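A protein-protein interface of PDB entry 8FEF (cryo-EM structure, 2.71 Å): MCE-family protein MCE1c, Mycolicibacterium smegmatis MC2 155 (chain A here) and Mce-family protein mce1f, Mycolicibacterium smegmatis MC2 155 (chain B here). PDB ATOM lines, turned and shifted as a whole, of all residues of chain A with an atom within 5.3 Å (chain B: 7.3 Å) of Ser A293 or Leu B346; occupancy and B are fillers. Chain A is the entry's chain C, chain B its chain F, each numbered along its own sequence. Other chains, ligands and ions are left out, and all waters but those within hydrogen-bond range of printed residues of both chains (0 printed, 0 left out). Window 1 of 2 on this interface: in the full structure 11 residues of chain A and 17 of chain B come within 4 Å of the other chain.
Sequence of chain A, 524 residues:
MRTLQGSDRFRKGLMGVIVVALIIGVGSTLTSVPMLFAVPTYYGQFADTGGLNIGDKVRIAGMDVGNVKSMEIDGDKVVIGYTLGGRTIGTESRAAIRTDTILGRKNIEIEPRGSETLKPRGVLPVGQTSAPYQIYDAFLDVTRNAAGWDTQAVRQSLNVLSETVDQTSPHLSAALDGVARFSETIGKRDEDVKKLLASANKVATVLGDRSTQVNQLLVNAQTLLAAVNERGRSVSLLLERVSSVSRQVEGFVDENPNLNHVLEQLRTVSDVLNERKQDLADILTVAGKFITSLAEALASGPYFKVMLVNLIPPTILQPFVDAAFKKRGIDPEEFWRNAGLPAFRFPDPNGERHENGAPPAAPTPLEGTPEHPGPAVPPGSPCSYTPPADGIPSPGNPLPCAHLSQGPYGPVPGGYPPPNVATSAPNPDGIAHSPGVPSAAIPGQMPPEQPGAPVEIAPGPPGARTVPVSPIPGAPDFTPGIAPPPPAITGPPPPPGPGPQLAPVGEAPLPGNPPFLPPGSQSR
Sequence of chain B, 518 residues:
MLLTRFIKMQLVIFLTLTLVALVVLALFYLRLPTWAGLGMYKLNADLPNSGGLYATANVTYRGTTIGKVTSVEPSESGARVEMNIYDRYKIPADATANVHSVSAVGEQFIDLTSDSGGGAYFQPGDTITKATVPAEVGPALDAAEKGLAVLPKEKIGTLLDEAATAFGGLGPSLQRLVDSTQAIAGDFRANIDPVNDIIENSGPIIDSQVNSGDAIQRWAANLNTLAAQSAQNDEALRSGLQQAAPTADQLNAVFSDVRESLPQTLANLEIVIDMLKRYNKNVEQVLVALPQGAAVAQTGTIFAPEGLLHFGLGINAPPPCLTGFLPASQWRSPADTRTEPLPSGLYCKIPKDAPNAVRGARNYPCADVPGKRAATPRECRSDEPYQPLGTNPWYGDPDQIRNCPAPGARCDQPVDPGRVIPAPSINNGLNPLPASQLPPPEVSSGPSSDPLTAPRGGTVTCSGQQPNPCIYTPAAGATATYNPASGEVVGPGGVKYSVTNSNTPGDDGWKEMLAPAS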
ATOM      1  N   PHE A 290      -7.109  -5.555  19.124  1.00  0.00           N
ATOM      2  CA  PHE A 290      -7.961  -5.313  17.964  1.00  0.00           C
ATOM      3  C   PHE A 290      -7.193  -5.081  16.675  1.00  0.00           C
ATOM      4  O   PHE A 290      -7.834  -4.953  15.629  1.00  0.00           O
ATOM      5  CB  PHE A 290      -8.921  -4.127  18.204  1.00  0.00           C
ATOM      6  CG  PHE A 290      -8.280  -2.758  18.104  1.00  0.00           C
ATOM      7  CD1 PHE A 290      -8.181  -2.092  16.891  1.00  0.00           C
ATOM      8  CD2 PHE A 290      -7.832  -2.116  19.238  1.00  0.00           C
ATOM      9  CE1 PHE A 290      -7.604  -0.843  16.813  1.00  0.00           C
ATOM     10  CE2 PHE A 290      -7.258  -0.865  19.165  1.00  0.00           C
ATOM     11  CZ  PHE A 290      -7.147  -0.226  17.952  1.00  0.00           C
ATOM     12  N   ILE A 291      -5.860  -5.008  16.703  1.00  0.00           N
ATOM     13  CA  ILE A 291      -5.107  -4.705  15.489  1.00  0.00           C
ATOM     14  C   ILE A 291      -5.305  -5.804  14.449  1.00  0.00           C
ATOM     15  O   ILE A 291      -5.439  -5.525  13.251  1.00  0.00           O
ATOM     16  CB  ILE A 291      -3.620  -4.475  15.826  1.00  0.00           C
ATOM     17  CG1 ILE A 291      -2.810  -4.215  14.557  1.00  0.00           C
ATOM     18  CG2 ILE A 291      -3.045  -5.635  16.622  1.00  0.00           C
ATOM     19  CD1 ILE A 291      -1.370  -3.877  14.826  1.00  0.00           C
ATOM     20  N   THR A 292      -5.354  -7.065  14.889  1.00  0.00           N
ATOM     21  CA  THR A 292      -5.607  -8.162  13.962  1.00  0.00           C
ATOM     22  C   THR A 292      -7.020  -8.105  13.401  1.00  0.00           C
ATOM     23  O   THR A 292      -7.242  -8.479  12.245  1.00  0.00           O
ATOM     24  CB  THR A 292      -5.373  -9.509  14.648  1.00  0.00           C
ATOM     25  OG1 THR A 292      -6.172  -9.587  15.836  1.00  0.00           O
ATOM     26  CG2 THR A 292      -3.907  -9.677  15.012  1.00  0.00           C
ATOM     27  N   SER A 293      -7.984  -7.649  14.203  1.00  0.00           N
ATOM     28  CA  SER A 293      -9.366  -7.583  13.741  1.00  0.00           C
ATOM     29  C   SER A 293      -9.566  -6.439  12.755  1.00  0.00           C
ATOM     30  O   SER A 293     -10.302  -6.581  11.771  1.00  0.00           O
ATOM     31  CB  SER A 293     -10.312  -7.438  14.930  1.00  0.00           C
ATOM     32  OG  SER A 293     -11.662  -7.442  14.503  1.00  0.00           O
ATOM     33  N   LEU A 294      -9.008  -5.271  13.056  1.00  0.00           N
ATOM     34  CA  LEU A 294      -9.173  -4.100  12.194  1.00  0.00           C
ATOM     35  C   LEU A 294      -8.409  -4.157  10.893  1.00  0.00           C
ATOM     36  O   LEU A 294      -8.743  -3.455   9.954  1.00  0.00           O
ATOM     37  CB  LEU A 294      -8.831  -2.809  12.923  1.00  0.00           C
ATOM     38  CG  LEU A 294     -10.055  -1.932  13.145  1.00  0.00           C
ATOM     39  CD1 LEU A 294     -11.089  -2.661  13.983  1.00  0.00           C
ATOM     40  CD2 LEU A 294      -9.657  -0.608  13.765  1.00  0.00           C
ATOM     41  N   ALA A 295      -7.374  -4.984  10.837  1.00  0.00           N
ATOM     42  CA  ALA A 295      -6.597  -5.138   9.623  1.00  0.00           C
ATOM     43  C   ALA A 295      -7.171  -6.250   8.755  1.00  0.00           C
ATOM     44  O   ALA A 295      -6.659  -6.519   7.682  1.00  0.00           O
ATOM     45  CB  ALA A 295      -5.147  -5.416   9.955  1.00  0.00           C
ATOM     46  N   GLU A 296      -8.183  -6.945   9.267  1.00  0.00           N
ATOM     47  CA  GLU A 296      -8.864  -8.014   8.557  1.00  0.00           C
ATOM     48  C   GLU A 296      -9.636  -7.495   7.355  1.00  0.00           C
ATOM     49  O   GLU A 296      -9.686  -8.142   6.315  1.00  0.00           O
ATOM     50  CB  GLU A 296      -9.782  -8.792   9.496  1.00  0.00           C
ATOM     51  CG  GLU A 296      -9.588 -10.295   9.417  1.00  0.00           C
ATOM     52  CD  GLU A 296      -8.130 -10.676   9.233  1.00  0.00           C
ATOM     53  OE1 GLU A 296      -7.253  -9.896   9.645  1.00  0.00           O
ATOM     54  OE2 GLU A 296      -7.850 -11.749   8.665  1.00  0.00           O
ATOM     55  N   ALA A 297     -10.245  -6.323   7.507  1.00  0.00           N
ATOM     56  CA  ALA A 297     -11.046  -5.713   6.455  1.00  0.00           C
ATOM     57  C   ALA A 297     -10.210  -5.428   5.236  1.00  0.00           C
ATOM     58  O   ALA A 297     -10.650  -5.641   4.124  1.00  0.00           O
ATOM     59  CB  ALA A 297     -11.682  -4.439   6.960  1.00  0.00           C
ATOM     60  N   THR B 323     -17.139 -15.711  10.037  1.00  0.00           N
ATOM     61  CA  THR B 323     -16.632 -16.819  10.832  1.00  0.00           C
ATOM     62  C   THR B 323     -15.467 -16.350  11.691  1.00  0.00           C
ATOM     63  O   THR B 323     -14.507 -15.762  11.182  1.00  0.00           O
ATOM     64  CB  THR B 323     -16.180 -17.968   9.933  1.00  0.00           C
ATOM     65  OG1 THR B 323     -15.154 -17.504   9.046  1.00  0.00           O
ATOM     66  CG2 THR B 323     -17.340 -18.488   9.119  1.00  0.00           C
ATOM     67  N   GLY B 324     -15.547 -16.625  12.989  1.00  0.00           N
ATOM     68  CA  GLY B 324     -14.556 -16.135  13.919  1.00  0.00           C
ATOM     69  C   GLY B 324     -14.783 -14.723  14.396  1.00  0.00           C
ATOM     70  O   GLY B 324     -13.934 -14.185  15.113  1.00  0.00           O
ATOM     71  N   PHE B 325     -15.895 -14.104  14.015  1.00  0.00           N
ATOM     72  CA  PHE B 325     -16.273 -12.772  14.449  1.00  0.00           C
ATOM     73  C   PHE B 325     -17.520 -12.861  15.320  1.00  0.00           C
ATOM     74  O   PHE B 325     -18.009 -13.947  15.640  1.00  0.00           O
ATOM     75  CB  PHE B 325     -16.507 -11.856  13.251  1.00  0.00           C
ATOM     76  CG  PHE B 325     -15.262 -11.517  12.490  1.00  0.00           C
ATOM     77  CD1 PHE B 325     -14.338 -10.631  13.011  1.00  0.00           C
ATOM     78  CD2 PHE B 325     -15.024 -12.068  11.246  1.00  0.00           C
ATOM     79  CE1 PHE B 325     -13.198 -10.309  12.309  1.00  0.00           C
ATOM     80  CE2 PHE B 325     -13.885 -11.749  10.540  1.00  0.00           C
ATOM     81  CZ  PHE B 325     -12.971 -10.869  11.072  1.00  0.00           C
ATOM     82  N   LEU B 326     -18.030 -11.699  15.707  1.00  0.00           N
ATOM     83  CA  LEU B 326     -19.173 -11.647  16.604  1.00  0.00           C
ATOM     84  C   LEU B 326     -20.416 -12.204  15.910  1.00  0.00           C
ATOM     85  O   LEU B 326     -20.606 -11.989  14.711  1.00  0.00           O
ATOM     86  CB  LEU B 326     -19.419 -10.207  17.053  1.00  0.00           C
ATOM     87  CG  LEU B 326     -20.045  -9.968  18.425  1.00  0.00           C
ATOM     88  CD1 LEU B 326     -19.176 -10.566  19.515  1.00  0.00           C
ATOM     89  CD2 LEU B 326     -20.247  -8.480  18.653  1.00  0.00           C
ATOM     90  N   PRO B 327     -21.268 -12.930  16.629  1.00  0.00           N
ATOM     91  CA  PRO B 327     -22.494 -13.452  16.018  1.00  0.00           C
ATOM     92  C   PRO B 327     -23.450 -12.333  15.636  1.00  0.00           C
ATOM     93  O   PRO B 327     -23.361 -11.205  16.123  1.00  0.00           O
ATOM     94  CB  PRO B 327     -23.093 -14.339  17.114  1.00  0.00           C
ATOM     95  CG  PRO B 327     -21.950 -14.666  18.008  1.00  0.00           C
ATOM     96  CD  PRO B 327     -21.065 -13.460  17.987  1.00  0.00           C
ATOM     97  N   LEU B 342     -13.958  -4.179  24.055  1.00  0.00           N
ATOM     98  CA  LEU B 342     -13.681  -4.793  22.763  1.00  0.00           C
ATOM     99  C   LEU B 342     -13.333  -6.267  22.937  1.00  0.00           C
ATOM    100  O   LEU B 342     -12.539  -6.611  23.818  1.00  0.00           O
ATOM    101  CB  LEU B 342     -12.545  -4.057  22.043  1.00  0.00           C
ATOM    102  CG  LEU B 342     -11.133  -3.918  22.623  1.00  0.00           C
ATOM    103  CD1 LEU B 342     -10.199  -3.471  21.528  1.00  0.00           C
ATOM    104  CD2 LEU B 342     -11.057  -2.933  23.776  1.00  0.00           C
ATOM    105  N   PRO B 343     -13.916  -7.158  22.140  1.00  0.00           N
ATOM    106  CA  PRO B 343     -13.631  -8.588  22.288  1.00  0.00           C
ATOM    107  C   PRO B 343     -12.229  -8.933  21.810  1.00  0.00           C
ATOM    108  O   PRO B 343     -11.591  -8.195  21.058  1.00  0.00           O
ATOM    109  CB  PRO B 343     -14.695  -9.261  21.413  1.00  0.00           C
ATOM    110  CG  PRO B 343     -15.718  -8.203  21.141  1.00  0.00           C
ATOM    111  CD  PRO B 343     -14.968  -6.911  21.142  1.00  0.00           C
ATOM    112  N   SER B 344     -11.755 -10.089  22.262  1.00  0.00           N
ATOM    113  CA  SER B 344     -10.418 -10.568  21.953  1.00  0.00           C
ATOM    114  C   SER B 344     -10.489 -11.823  21.093  1.00  0.00           C
ATOM    115  O   SER B 344     -11.420 -12.624  21.209  1.00  0.00           O
ATOM    116  CB  SER B 344      -9.633 -10.860  23.235  1.00  0.00           C
ATOM    117  OG  SER B 344      -8.315 -11.289  22.940  1.00  0.00           O
ATOM    118  N   GLY B 345      -9.488 -11.984  20.230  1.00  0.00           N
ATOM    119  CA  GLY B 345      -9.392 -13.152  19.377  1.00  0.00           C
ATOM    120  C   GLY B 345     -10.499 -13.285  18.351  1.00  0.00           C
ATOM    121  O   GLY B 345     -11.073 -14.365  18.189  1.00  0.00           O
ATOM    122  N   LEU B 346     -10.812 -12.196  17.655  1.00  0.00           N
ATOM    123  CA  LEU B 346     -11.800 -12.197  16.584  1.00  0.00           C
ATOM    124  C   LEU B 346     -11.101 -11.928  15.258  1.00  0.00           C
ATOM    125  O   LEU B 346     -10.549 -10.841  15.058  1.00  0.00           O
ATOM    126  CB  LEU B 346     -12.884 -11.149  16.831  1.00  0.00           C
ATOM    127  CG  LEU B 346     -13.839 -11.361  18.004  1.00  0.00           C
ATOM    128  CD1 LEU B 346     -14.975 -10.360  17.936  1.00  0.00           C
ATOM    129  CD2 LEU B 346     -14.374 -12.780  18.034  1.00  0.00           C
ATOM    130  N   TYR B 347     -11.128 -12.911  14.361  1.00  0.00           N
ATOM    131  CA  TYR B 347     -10.641 -12.715  13.001  1.00  0.00           C
ATOM    132  C   TYR B 347     -11.260 -13.773  12.096  1.00  0.00           C
ATOM    133  O   TYR B 347     -11.891 -14.726  12.559  1.00  0.00           O
ATOM    134  CB  TYR B 347      -9.108 -12.745  12.934  1.00  0.00           C
ATOM    135  CG  TYR B 347      -8.471 -14.064  13.300  1.00  0.00           C
ATOM    136  CD1 TYR B 347      -8.313 -14.438  14.624  1.00  0.00           C
ATOM    137  CD2 TYR B 347      -8.003 -14.925  12.316  1.00  0.00           C
ATOM    138  CE1 TYR B 347      -7.722 -15.640  14.961  1.00  0.00           C
ATOM    139  CE2 TYR B 347      -7.412 -16.129  12.643  1.00  0.00           C
ATOM    140  CZ  TYR B 347      -7.277 -16.483  13.967  1.00  0.00           C
ATOM    141  OH  TYR B 347      -6.686 -17.679  14.300  1.00  0.00           O
ATOM    142  N   CYS B 348     -11.092 -13.566  10.791  1.00  0.00           N
ATOM    143  CA  CYS B 348     -11.676 -14.435   9.774  1.00  0.00           C
ATOM    144  C   CYS B 348     -11.069 -15.831   9.858  1.00  0.00           C
ATOM    145  O   CYS B 348      -9.869 -16.010   9.629  1.00  0.00           O
ATOM    146  CB  CYS B 348     -11.445 -13.812   8.396  1.00  0.00           C
ATOM    147  SG  CYS B 348     -12.226 -14.584   6.954  1.00  0.00           S
ATOM    148  N   LYS B 349     -11.900 -16.821  10.184  1.00  0.00           N
ATOM    149  CA  LYS B 349     -11.452 -18.178  10.488  1.00  0.00           C
ATOM    150  C   LYS B 349     -11.737 -19.164   9.358  1.00  0.00           C
ATOM    151  O   LYS B 349     -12.098 -20.316   9.607  1.00  0.00           O
ATOM    152  CB  LYS B 349     -12.103 -18.684  11.771  1.00  0.00           C
ATOM    153  CG  LYS B 349     -11.661 -17.998  13.047  1.00  0.00           C
ATOM    154  CD  LYS B 349     -10.248 -18.359  13.436  1.00  0.00           C
ATOM    155  CE  LYS B 349     -10.080 -18.275  14.941  1.00  0.00           C
ATOM    156  NZ  LYS B 349     -10.583 -16.983  15.476  1.00  0.00           N
ATOM    157  N   ALA B 361      -5.429 -12.384   9.127  1.00  0.00           N
ATOM    158  CA  ALA B 361      -4.543 -12.637  10.258  1.00  0.00           C
ATOM    159  C   ALA B 361      -3.955 -14.040  10.207  1.00  0.00           C
ATOM    160  O   ALA B 361      -2.776 -14.236  10.518  1.00  0.00           O
ATOM    161  CB  ALA B 361      -5.293 -12.421  11.571  1.00  0.00           C
ATOM    162  N   TYR B 364      -0.512 -14.364   8.476  1.00  0.00           N
ATOM    163  CA  TYR B 364       0.633 -13.524   8.815  1.00  0.00           C
ATOM    164  C   TYR B 364       1.828 -14.405   9.152  1.00  0.00           C
ATOM    165  O   TYR B 364       1.690 -15.347   9.938  1.00  0.00           O
ATOM    166  CB  TYR B 364       0.318 -12.612   9.999  1.00  0.00           C
ATOM    167  CG  TYR B 364      -0.690 -11.521   9.730  1.00  0.00           C
ATOM    168  CD1 TYR B 364      -1.092 -11.215   8.439  1.00  0.00           C
ATOM    169  CD2 TYR B 364      -1.235 -10.790  10.773  1.00  0.00           C
ATOM    170  CE1 TYR B 364      -2.019 -10.221   8.201  1.00  0.00           C
ATOM    171  CE2 TYR B 364      -2.157  -9.792  10.543  1.00  0.00           C
ATOM    172  CZ  TYR B 364      -2.543  -9.508   9.256  1.00  0.00           C
ATOM    173  OH  TYR B 364      -3.463  -8.513   9.029  1.00  0.00           O
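Among the printed residues, pairs that only touch across the chains: Ser A293 with Leu B346 (3.4 Å), Phe A290 with Leu B342 (3.6 Å), Ala A295 with Tyr B364 (3.6 Å), Glu A296 with Phe B325 (3.8 Å), Glu A296 with Cys B348 (3.9 Å) and Ser A293 with Phe B325 (3.9 Å).
Of the 8 printed residues of chain A, 4 touch a printed residue of chain B.
Hydrophobic or aromatic side chains of chain A within 4 Å of the printed part of chain B: Phe A290 and Ala A295.
Hydrophobic or aromatic side chains of chain B that line the printed part of chain A: Phe B325, Leu B342, Ala B361 and Tyr B364.
Among the printed residues, 7 pairs touch across the chains.
Among the printed residues, no Asp or Glu carboxylate lies within 4 Å of a Lys or Arg side-chain nitrogen of the other chain.
N of Ala B361 is in hydrogen-bond range of OE2 of Glu A296, 2.5 Å away.
Of the printed residues of chain B, Phe A290 touches Leu B342.
Of chain B, only Phe B325 (3.9 Å) and Leu B346 (3.4 Å) come within 4 Å of Ser A293.
Printed residues of chain B within 4 Å of Glu A296: Phe B325, Cys B348 and Ala B361.
Of the printed residues of chain A, Phe B325 touches Ser A293 and Glu A296.
Gly B345 touches none of the printed residues of chain A.
Leu B346 touches just one residue of chain A: Ser A293 (3.4 Å).
Tyr B347 touches none of the printed residues of chain A.
Of the printed residues of chain A, Cys B348 touches Glu A296.
Printed residues of chain A within 4 Å of Tyr B364: Ala A295.
The nearest residue of chain B that does not touch Ser A293 is Tyr B347 (5.2 Å).
The nearest printed residue of chain A that does not touch Ala B361 is Thr A292 (4.2 Å).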
